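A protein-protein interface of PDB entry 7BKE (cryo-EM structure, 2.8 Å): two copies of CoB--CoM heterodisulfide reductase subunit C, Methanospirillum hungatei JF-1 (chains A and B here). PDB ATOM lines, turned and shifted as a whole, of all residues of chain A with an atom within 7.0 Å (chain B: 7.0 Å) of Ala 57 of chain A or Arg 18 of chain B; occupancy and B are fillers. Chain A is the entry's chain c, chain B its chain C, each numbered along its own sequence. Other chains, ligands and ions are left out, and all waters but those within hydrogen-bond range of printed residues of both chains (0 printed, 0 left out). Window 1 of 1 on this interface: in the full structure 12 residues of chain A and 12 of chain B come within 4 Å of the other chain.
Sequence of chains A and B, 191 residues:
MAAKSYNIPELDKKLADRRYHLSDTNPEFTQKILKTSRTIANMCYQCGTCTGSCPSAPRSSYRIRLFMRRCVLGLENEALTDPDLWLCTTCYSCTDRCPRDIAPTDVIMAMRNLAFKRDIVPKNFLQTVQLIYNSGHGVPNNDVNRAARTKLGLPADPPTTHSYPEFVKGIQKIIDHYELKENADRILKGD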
ATOM      1  N   CYS A  50     -14.391  -7.309  -5.083  1.00  0.00           N
ATOM      2  CA  CYS A  50     -14.882  -6.667  -3.872  1.00  0.00           C
ATOM      3  C   CYS A  50     -13.746  -6.103  -3.025  1.00  0.00           C
ATOM      4  O   CYS A  50     -13.770  -4.932  -2.625  1.00  0.00           O
ATOM      5  CB  CYS A  50     -15.735  -7.668  -3.098  1.00  0.00           C
ATOM      6  SG  CYS A  50     -14.982  -9.265  -2.823  1.00  0.00           S
ATOM      7  N   THR A  51     -12.729  -6.917  -2.746  1.00  0.00           N
ATOM      8  CA  THR A  51     -11.586  -6.432  -1.987  1.00  0.00           C
ATOM      9  C   THR A  51     -10.823  -5.368  -2.760  1.00  0.00           C
ATOM     10  O   THR A  51     -10.311  -4.415  -2.172  1.00  0.00           O
ATOM     11  CB  THR A  51     -10.662  -7.586  -1.625  1.00  0.00           C
ATOM     12  OG1 THR A  51     -11.413  -8.601  -0.963  1.00  0.00           O
ATOM     13  CG2 THR A  51      -9.568  -7.116  -0.707  1.00  0.00           C
ATOM     14  N   GLY A  52     -10.728  -5.517  -4.079  1.00  0.00           N
ATOM     15  CA  GLY A  52     -10.050  -4.510  -4.865  1.00  0.00           C
ATOM     16  C   GLY A  52     -10.739  -3.169  -4.858  1.00  0.00           C
ATOM     17  O   GLY A  52     -10.098  -2.153  -5.129  1.00  0.00           O
ATOM     18  N   SER A  53     -12.034  -3.144  -4.569  1.00  0.00           N
ATOM     19  CA  SER A  53     -12.773  -1.893  -4.506  1.00  0.00           C
ATOM     20  C   SER A  53     -12.966  -1.355  -3.094  1.00  0.00           C
ATOM     21  O   SER A  53     -13.334  -0.189  -2.949  1.00  0.00           O
ATOM     22  CB  SER A  53     -14.142  -2.066  -5.166  1.00  0.00           C
ATOM     23  OG  SER A  53     -14.753  -3.264  -4.751  1.00  0.00           O
ATOM     24  N   CYS A  54     -12.750  -2.169  -2.065  1.00  0.00           N
ATOM     25  CA  CYS A  54     -13.009  -1.731  -0.698  1.00  0.00           C
ATOM     26  C   CYS A  54     -12.101  -0.574  -0.285  1.00  0.00           C
ATOM     27  O   CYS A  54     -10.894  -0.626  -0.535  1.00  0.00           O
ATOM     28  CB  CYS A  54     -12.827  -2.893   0.270  1.00  0.00           C
ATOM     29  SG  CYS A  54     -13.405  -2.578   1.928  1.00  0.00           S
ATOM     30  N   PRO A  55     -12.637   0.474   0.351  1.00  0.00           N
ATOM     31  CA  PRO A  55     -11.775   1.529   0.896  1.00  0.00           C
ATOM     32  C   PRO A  55     -11.189   1.209   2.259  1.00  0.00           C
ATOM     33  O   PRO A  55     -10.269   1.910   2.689  1.00  0.00           O
ATOM     34  CB  PRO A  55     -12.717   2.727   0.985  1.00  0.00           C
ATOM     35  CG  PRO A  55     -14.018   2.122   1.241  1.00  0.00           C
ATOM     36  CD  PRO A  55     -14.055   0.829   0.478  1.00  0.00           C
ATOM     37  N   SER A  56     -11.697   0.188   2.950  1.00  0.00           N
ATOM     38  CA  SER A  56     -11.140  -0.211   4.233  1.00  0.00           C
ATOM     39  C   SER A  56      -9.965  -1.167   4.086  1.00  0.00           C
ATOM     40  O   SER A  56      -9.137  -1.260   4.993  1.00  0.00           O
ATOM     41  CB  SER A  56     -12.215  -0.871   5.092  1.00  0.00           C
ATOM     42  OG  SER A  56     -13.047   0.092   5.700  1.00  0.00           O
ATOM     43  N   ALA A  57      -9.892  -1.897   2.979  1.00  0.00           N
ATOM     44  CA  ALA A  57      -8.836  -2.887   2.804  1.00  0.00           C
ATOM     45  C   ALA A  57      -7.422  -2.311   2.784  1.00  0.00           C
ATOM     46  O   ALA A  57      -6.533  -2.940   3.378  1.00  0.00           O
ATOM     47  CB  ALA A  57      -9.104  -3.706   1.538  1.00  0.00           C
ATOM     48  N   PRO A  58      -7.128  -1.185   2.126  1.00  0.00           N
ATOM     49  CA  PRO A  58      -5.731  -0.734   2.036  1.00  0.00           C
ATOM     50  C   PRO A  58      -5.111  -0.310   3.356  1.00  0.00           C
ATOM     51  O   PRO A  58      -3.908  -0.039   3.378  1.00  0.00           O
ATOM     52  CB  PRO A  58      -5.808   0.460   1.079  1.00  0.00           C
ATOM     53  CG  PRO A  58      -7.074   0.325   0.395  1.00  0.00           C
ATOM     54  CD  PRO A  58      -8.006  -0.307   1.335  1.00  0.00           C
ATOM     55  N   ARG A  59      -5.876  -0.216   4.441  1.00  0.00           N
ATOM     56  CA  ARG A  59      -5.357   0.313   5.695  1.00  0.00           C
ATOM     57  C   ARG A  59      -5.645  -0.605   6.872  1.00  0.00           C
ATOM     58  O   ARG A  59      -5.558  -0.169   8.016  1.00  0.00           O
ATOM     59  CB  ARG A  59      -5.939   1.691   5.989  1.00  0.00           C
ATOM     60  CG  ARG A  59      -7.443   1.684   6.035  1.00  0.00           C
ATOM     61  CD  ARG A  59      -7.988   3.065   5.992  1.00  0.00           C
ATOM     62  NE  ARG A  59      -7.235   3.883   5.062  1.00  0.00           N
ATOM     63  CZ  ARG A  59      -7.501   4.004   3.774  1.00  0.00           C
ATOM     64  NH1 ARG A  59      -8.508   3.350   3.223  1.00  0.00           N
ATOM     65  NH2 ARG A  59      -6.741   4.782   3.036  1.00  0.00           N
ATOM     66  N   SER A  60      -6.008  -1.848   6.622  1.00  0.00           N
ATOM     67  CA  SER A  60      -6.373  -2.745   7.701  1.00  0.00           C
ATOM     68  C   SER A  60      -6.228  -4.168   7.193  1.00  0.00           C
ATOM     69  O   SER A  60      -5.782  -4.399   6.066  1.00  0.00           O
ATOM     70  CB  SER A  60      -7.786  -2.444   8.195  1.00  0.00           C
ATOM     71  OG  SER A  60      -8.746  -2.793   7.224  1.00  0.00           O
ATOM     72  N   SER A  61      -6.607  -5.127   8.025  1.00  0.00           N
ATOM     73  CA  SER A  61      -6.629  -6.524   7.636  1.00  0.00           C
ATOM     74  C   SER A  61      -8.000  -6.966   7.152  1.00  0.00           C
ATOM     75  O   SER A  61      -8.216  -8.161   6.940  1.00  0.00           O
ATOM     76  CB  SER A  61      -6.171  -7.397   8.802  1.00  0.00           C
ATOM     77  OG  SER A  61      -7.101  -7.365   9.866  1.00  0.00           O
ATOM     78  N   TYR A  62      -8.929  -6.031   6.972  1.00  0.00           N
ATOM     79  CA  TYR A  62     -10.280  -6.361   6.541  1.00  0.00           C
ATOM     80  C   TYR A  62     -10.279  -6.839   5.096  1.00  0.00           C
ATOM     81  O   TYR A  62      -9.785  -6.146   4.204  1.00  0.00           O
ATOM     82  CB  TYR A  62     -11.178  -5.138   6.708  1.00  0.00           C
ATOM     83  CG  TYR A  62     -12.581  -5.315   6.198  1.00  0.00           C
ATOM     84  CD1 TYR A  62     -13.406  -6.282   6.725  1.00  0.00           C
ATOM     85  CD2 TYR A  62     -13.076  -4.513   5.189  1.00  0.00           C
ATOM     86  CE1 TYR A  62     -14.677  -6.448   6.266  1.00  0.00           C
ATOM     87  CE2 TYR A  62     -14.344  -4.677   4.725  1.00  0.00           C
ATOM     88  CZ  TYR A  62     -15.140  -5.647   5.264  1.00  0.00           C
ATOM     89  OH  TYR A  62     -16.412  -5.814   4.800  1.00  0.00           O
ATOM     90  N   ARG A  63     -10.824  -8.032   4.863  1.00  0.00           N
ATOM     91  CA  ARG A  63     -10.922  -8.619   3.526  1.00  0.00           C
ATOM     92  C   ARG A  63     -12.343  -9.136   3.326  1.00  0.00           C
ATOM     93  O   ARG A  63     -12.725 -10.183   3.863  1.00  0.00           O
ATOM     94  CB  ARG A  63      -9.903  -9.730   3.323  1.00  0.00           C
ATOM     95  CG  ARG A  63      -8.463  -9.316   3.498  1.00  0.00           C
ATOM     96  CD  ARG A  63      -7.997  -8.417   2.386  1.00  0.00           C
ATOM     97  NE  ARG A  63      -6.622  -7.985   2.596  1.00  0.00           N
ATOM     98  CZ  ARG A  63      -6.275  -6.866   3.221  1.00  0.00           C
ATOM     99  NH1 ARG A  63      -7.204  -6.056   3.696  1.00  0.00           N
ATOM    100  NH2 ARG A  63      -4.999  -6.557   3.370  1.00  0.00           N
ATOM    101  N   ILE A  64     -13.122  -8.399   2.539  1.00  0.00           N
ATOM    102  CA  ILE A  64     -14.503  -8.788   2.300  1.00  0.00           C
ATOM    103  C   ILE A  64     -14.571 -10.102   1.533  1.00  0.00           C
ATOM    104  O   ILE A  64     -15.471 -10.912   1.763  1.00  0.00           O
ATOM    105  CB  ILE A  64     -15.249  -7.646   1.586  1.00  0.00           C
ATOM    106  CG1 ILE A  64     -16.675  -8.056   1.252  1.00  0.00           C
ATOM    107  CG2 ILE A  64     -14.520  -7.192   0.352  1.00  0.00           C
ATOM    108  CD1 ILE A  64     -17.454  -8.486   2.437  1.00  0.00           C
ATOM    109  N   LEU A  87     -15.371  -2.882  10.325  1.00  0.00           N
ATOM    110  CA  LEU A  87     -14.654  -1.895   9.536  1.00  0.00           C
ATOM    111  C   LEU A  87     -15.284  -1.656   8.174  1.00  0.00           C
ATOM    112  O   LEU A  87     -14.734  -0.894   7.381  1.00  0.00           O
ATOM    113  CB  LEU A  87     -13.194  -2.313   9.365  1.00  0.00           C
ATOM    114  CG  LEU A  87     -12.309  -2.300  10.607  1.00  0.00           C
ATOM    115  CD1 LEU A  87     -10.960  -2.873  10.267  1.00  0.00           C
ATOM    116  CD2 LEU A  87     -12.169  -0.901  11.140  1.00  0.00           C
ATOM    117  N   ALA B   2      -3.288   4.736   5.697  1.00  0.00           N
ATOM    118  CA  ALA B   2      -2.514   4.526   4.483  1.00  0.00           C
ATOM    119  C   ALA B   2      -2.481   5.787   3.630  1.00  0.00           C
ATOM    120  O   ALA B   2      -2.034   5.758   2.486  1.00  0.00           O
ATOM    121  CB  ALA B   2      -3.082   3.365   3.685  1.00  0.00           C
ATOM    122  N   ASP B  12       1.270   4.594  12.545  1.00  0.00           N
ATOM    123  CA  ASP B  12       1.893   4.084  11.330  1.00  0.00           C
ATOM    124  C   ASP B  12       1.783   2.568  11.254  1.00  0.00           C
ATOM    125  O   ASP B  12       1.498   2.009  10.189  1.00  0.00           O
ATOM    126  CB  ASP B  12       3.351   4.529  11.260  1.00  0.00           C
ATOM    127  CG  ASP B  12       3.489   6.031  11.108  1.00  0.00           C
ATOM    128  OD1 ASP B  12       2.462   6.695  10.861  1.00  0.00           O
ATOM    129  OD2 ASP B  12       4.618   6.545  11.231  1.00  0.00           O
ATOM    130  N   LYS B  13       1.980   1.887  12.383  1.00  0.00           N
ATOM    131  CA  LYS B  13       1.809   0.442  12.419  1.00  0.00           C
ATOM    132  C   LYS B  13       0.366   0.042  12.133  1.00  0.00           C
ATOM    133  O   LYS B  13       0.114  -0.959  11.454  1.00  0.00           O
ATOM    134  CB  LYS B  13       2.256  -0.101  13.773  1.00  0.00           C
ATOM    135  CG  LYS B  13       2.166  -1.609  13.894  1.00  0.00           C
ATOM    136  CD  LYS B  13       2.729  -2.093  15.218  1.00  0.00           C
ATOM    137  CE  LYS B  13       2.500  -3.583  15.406  1.00  0.00           C
ATOM    138  NZ  LYS B  13       3.253  -4.412  14.430  1.00  0.00           N
ATOM    139  N   LYS B  14      -0.595   0.806  12.654  1.00  0.00           N
ATOM    140  CA  LYS B  14      -2.000   0.445  12.491  1.00  0.00           C
ATOM    141  C   LYS B  14      -2.492   0.714  11.074  1.00  0.00           C
ATOM    142  O   LYS B  14      -3.268  -0.072  10.523  1.00  0.00           O
ATOM    143  CB  LYS B  14      -2.853   1.204  13.501  1.00  0.00           C
ATOM    144  CG  LYS B  14      -4.291   0.752  13.548  1.00  0.00           C
ATOM    145  CD  LYS B  14      -5.101   1.607  14.499  1.00  0.00           C
ATOM    146  CE  LYS B  14      -6.402   2.041  13.864  1.00  0.00           C
ATOM    147  NZ  LYS B  14      -7.327   0.894  13.683  1.00  0.00           N
ATOM    148  N   LEU B  15      -2.059   1.818  10.472  1.00  0.00           N
ATOM    149  CA  LEU B  15      -2.494   2.220   9.142  1.00  0.00           C
ATOM    150  C   LEU B  15      -1.398   2.034   8.100  1.00  0.00           C
ATOM    151  O   LEU B  15      -1.318   2.798   7.138  1.00  0.00           O
ATOM    152  CB  LEU B  15      -2.966   3.671   9.149  1.00  0.00           C
ATOM    153  CG  LEU B  15      -3.861   4.140  10.290  1.00  0.00           C
ATOM    154  CD1 LEU B  15      -4.042   5.640  10.214  1.00  0.00           C
ATOM    155  CD2 LEU B  15      -5.201   3.433  10.264  1.00  0.00           C
ATOM    156  N   ALA B  16      -0.530   1.046   8.295  1.00  0.00           N
ATOM    157  CA  ALA B  16       0.436   0.693   7.267  1.00  0.00           C
ATOM    158  C   ALA B  16      -0.269   0.395   5.954  1.00  0.00           C
ATOM    159  O   ALA B  16      -1.296  -0.286   5.924  1.00  0.00           O
ATOM    160  CB  ALA B  16       1.255  -0.518   7.705  1.00  0.00           C
ATOM    161  N   ASP B  17       0.277   0.927   4.865  1.00  0.00           N
ATOM    162  CA  ASP B  17      -0.272   0.661   3.543  1.00  0.00           C
ATOM    163  C   ASP B  17      -0.164  -0.823   3.225  1.00  0.00           C
ATOM    164  O   ASP B  17       0.940  -1.357   3.098  1.00  0.00           O
ATOM    165  CB  ASP B  17       0.451   1.497   2.489  1.00  0.00           C
ATOM    166  CG  ASP B  17      -0.339   1.622   1.202  1.00  0.00           C
ATOM    167  OD1 ASP B  17      -1.514   1.213   1.179  1.00  0.00           O
ATOM    168  OD2 ASP B  17       0.219   2.133   0.209  1.00  0.00           O
ATOM    169  N   ARG B  18      -1.301  -1.496   3.104  1.00  0.00           N
ATOM    170  CA  ARG B  18      -1.350  -2.920   2.809  1.00  0.00           C
ATOM    171  C   ARG B  18      -1.370  -3.211   1.319  1.00  0.00           C
ATOM    172  O   ARG B  18      -1.473  -4.376   0.930  1.00  0.00           O
ATOM    173  CB  ARG B  18      -2.584  -3.547   3.456  1.00  0.00           C
ATOM    174  CG  ARG B  18      -2.303  -4.260   4.753  1.00  0.00           C
ATOM    175  CD  ARG B  18      -2.177  -3.276   5.885  1.00  0.00           C
ATOM    176  NE  ARG B  18      -2.618  -3.837   7.152  1.00  0.00           N
ATOM    177  CZ  ARG B  18      -2.839  -3.113   8.242  1.00  0.00           C
ATOM    178  NH1 ARG B  18      -2.658  -1.804   8.210  1.00  0.00           N
ATOM    179  NH2 ARG B  18      -3.243  -3.698   9.359  1.00  0.00           N
ATOM    180  N   ARG B  19      -1.262  -2.191   0.485  1.00  0.00           N
ATOM    181  CA  ARG B  19      -1.544  -2.299  -0.936  1.00  0.00           C
ATOM    182  C   ARG B  19      -0.238  -2.421  -1.708  1.00  0.00           C
ATOM    183  O   ARG B  19       0.642  -1.566  -1.585  1.00  0.00           O
ATOM    184  CB  ARG B  19      -2.346  -1.082  -1.388  1.00  0.00           C
ATOM    185  CG  ARG B  19      -2.820  -1.112  -2.800  1.00  0.00           C
ATOM    186  CD  ARG B  19      -3.517   0.186  -3.133  1.00  0.00           C
ATOM    187  NE  ARG B  19      -4.968   0.086  -3.058  1.00  0.00           N
ATOM    188  CZ  ARG B  19      -5.764   1.128  -2.871  1.00  0.00           C
ATOM    189  NH1 ARG B  19      -5.246   2.338  -2.728  1.00  0.00           N
ATOM    190  NH2 ARG B  19      -7.074   0.963  -2.820  1.00  0.00           N
ATOM    191  N   TYR B  20      -0.118  -3.480  -2.502  1.00  0.00           N
ATOM    192  CA  TYR B  20       1.100  -3.725  -3.262  1.00  0.00           C
ATOM    193  C   TYR B  20       1.236  -2.724  -4.401  1.00  0.00           C
ATOM    194  O   TYR B  20       0.309  -2.533  -5.188  1.00  0.00           O
ATOM    195  CB  TYR B  20       1.095  -5.155  -3.810  1.00  0.00           C
ATOM    196  CG  TYR B  20       2.162  -5.419  -4.850  1.00  0.00           C
ATOM    197  CD1 TYR B  20       3.455  -5.740  -4.478  1.00  0.00           C
ATOM    198  CD2 TYR B  20       1.873  -5.343  -6.205  1.00  0.00           C
ATOM    199  CE1 TYR B  20       4.427  -5.974  -5.419  1.00  0.00           C
ATOM    200  CE2 TYR B  20       2.843  -5.574  -7.152  1.00  0.00           C
ATOM    201  CZ  TYR B  20       4.117  -5.889  -6.754  1.00  0.00           C
ATOM    202  OH  TYR B  20       5.085  -6.124  -7.698  1.00  0.00           O
ATOM    203  N   HIS B  21       2.398  -2.090  -4.487  1.00  0.00           N
ATOM    204  CA  HIS B  21       2.740  -1.186  -5.570  1.00  0.00           C
ATOM    205  C   HIS B  21       3.884  -1.779  -6.375  1.00  0.00           C
ATOM    206  O   HIS B  21       4.611  -2.655  -5.901  1.00  0.00           O
ATOM    207  CB  HIS B  21       3.150   0.191  -5.042  1.00  0.00           C
ATOM    208  CG  HIS B  21       2.022   0.970  -4.453  1.00  0.00           C
ATOM    209  ND1 HIS B  21       1.813   1.060  -3.096  1.00  0.00           N
ATOM    210  CD2 HIS B  21       1.037   1.691  -5.037  1.00  0.00           C
ATOM    211  CE1 HIS B  21       0.747   1.804  -2.867  1.00  0.00           C
ATOM    212  NE2 HIS B  21       0.258   2.200  -4.028  1.00  0.00           N
ATOM    213  N   ASP B  24       7.382  -1.754  -4.941  1.00  0.00           N
ATOM    214  CA  ASP B  24       7.714  -2.746  -3.930  1.00  0.00           C
ATOM    215  C   ASP B  24       8.530  -3.905  -4.475  1.00  0.00           C
ATOM    216  O   ASP B  24       9.033  -4.711  -3.687  1.00  0.00           O
ATOM    217  CB  ASP B  24       6.432  -3.299  -3.301  1.00  0.00           C
ATOM    218  CG  ASP B  24       5.577  -2.220  -2.678  1.00  0.00           C
ATOM    219  OD1 ASP B  24       4.450  -2.530  -2.243  1.00  0.00           O
ATOM    220  OD2 ASP B  24       6.040  -1.064  -2.615  1.00  0.00           O
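No position is printed for both chains.
Of the 12 printed residues of chain B, 6 touch a printed residue of chain A. Of the 16 printed residues of chain A, 6 touch a printed residue of chain B. Hydrophobic or aromatic side chains of chain A that line the printed part of chain B: Pro 58. Among the printed residues, 12 pairs touch across the chains.
Ser 53 of chain A touches none of the printed residues of chain B. Of the printed residues of chain B, Ala 57 of chain A touches Arg 18. Printed residues of chain B within 4 Å of Pro 58 of chain A: Ala 2, Ala 16, Asp 17, Arg 18 and Arg 19. Printed residues of chain B within 4 Å of Ser 61 of chain A: Arg 18 (3.9 Å). Of the printed residues of chain A, Asp 17 of chain B touches Pro 58 (3.5 Å). Of the printed residues of chain A, Arg 18 of chain B touches Ala 57 (3.996 Å), Pro 58 (3.0 Å), Arg 59 (3.3 Å), Ser 60 (3.4 Å), Ser 61 (3.9 Å) and Arg 63 (3.8 Å). Of the printed residues of chain A, Arg 19 of chain B touches Pro 58.
The side-chain carboxylate of Asp 17 of chain B sits close to the backbone NH of Arg 19 of chain B, at 3.5 Å. The backbone carbonyl oxygen (O) of Arg 19 of chain B is in hydrogen-bond range of a ring nitrogen (ND1) of His 21 of chain B (3.2 Å). The backbone carbonyl oxygen of Ser 56 of chain A is in hydrogen-bond range of the side-chain hydroxyl of Ser 60 of chain A (2.7 Å). O of Ala 57 of chain A lies within hydrogen-bond range of NH1 of Arg 63 of chain A (3.2 Å). The side-chain hydroxyl of Ser 60 of chain A lies within hydrogen-bond range of the backbone NH of Tyr 62 of chain A (3.3 Å). The guanidinium group (NH1) of Arg 63 of chain A is in hydrogen-bond range of the backbone carbonyl oxygen (O) of Ser 60 of chain A, at 3.2 Å.
Among the printed residues, merely in contact across the chains: Ala 57 of chain A with Arg 18 of chain B (3.996 Å), Pro 58 of chain A with Ala 2 of chain B (3.5 Å), Pro 58 of chain A with Ala 16 of chain B (3.7 Å), Pro 58 of chain A with Arg 19 of chain B (3.3 Å), Arg 59 of chain A with Ala 2 of chain B (3.98 Å), Ser 61 of chain A with Arg 18 of chain B (3.9 Å) and Arg 63 of chain A with Arg 18 of chain B (3.8 Å).
The backbone carbonyl oxygen (O) of Pro 58 of chain A is in hydrogen-bond range of the backbone NH (N) of Arg 18 of chain B (3.0 Å). The guanidinium group (NH1) of Arg 18 of chain B is in hydrogen-bond range of the backbone carbonyl oxygen (O) of Arg 59 of chain A, at 3.3 Å. NE of Arg 18 of chain B lies within hydrogen-bond range of O of Ser 60 of chain A (3.4 Å). OD1 of Asp 17 of chain B lies close to O of Pro 58 of chain A. O of Lys 14 of chain B sits close to O of Arg 59 of chain A, 3.4 Å away.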
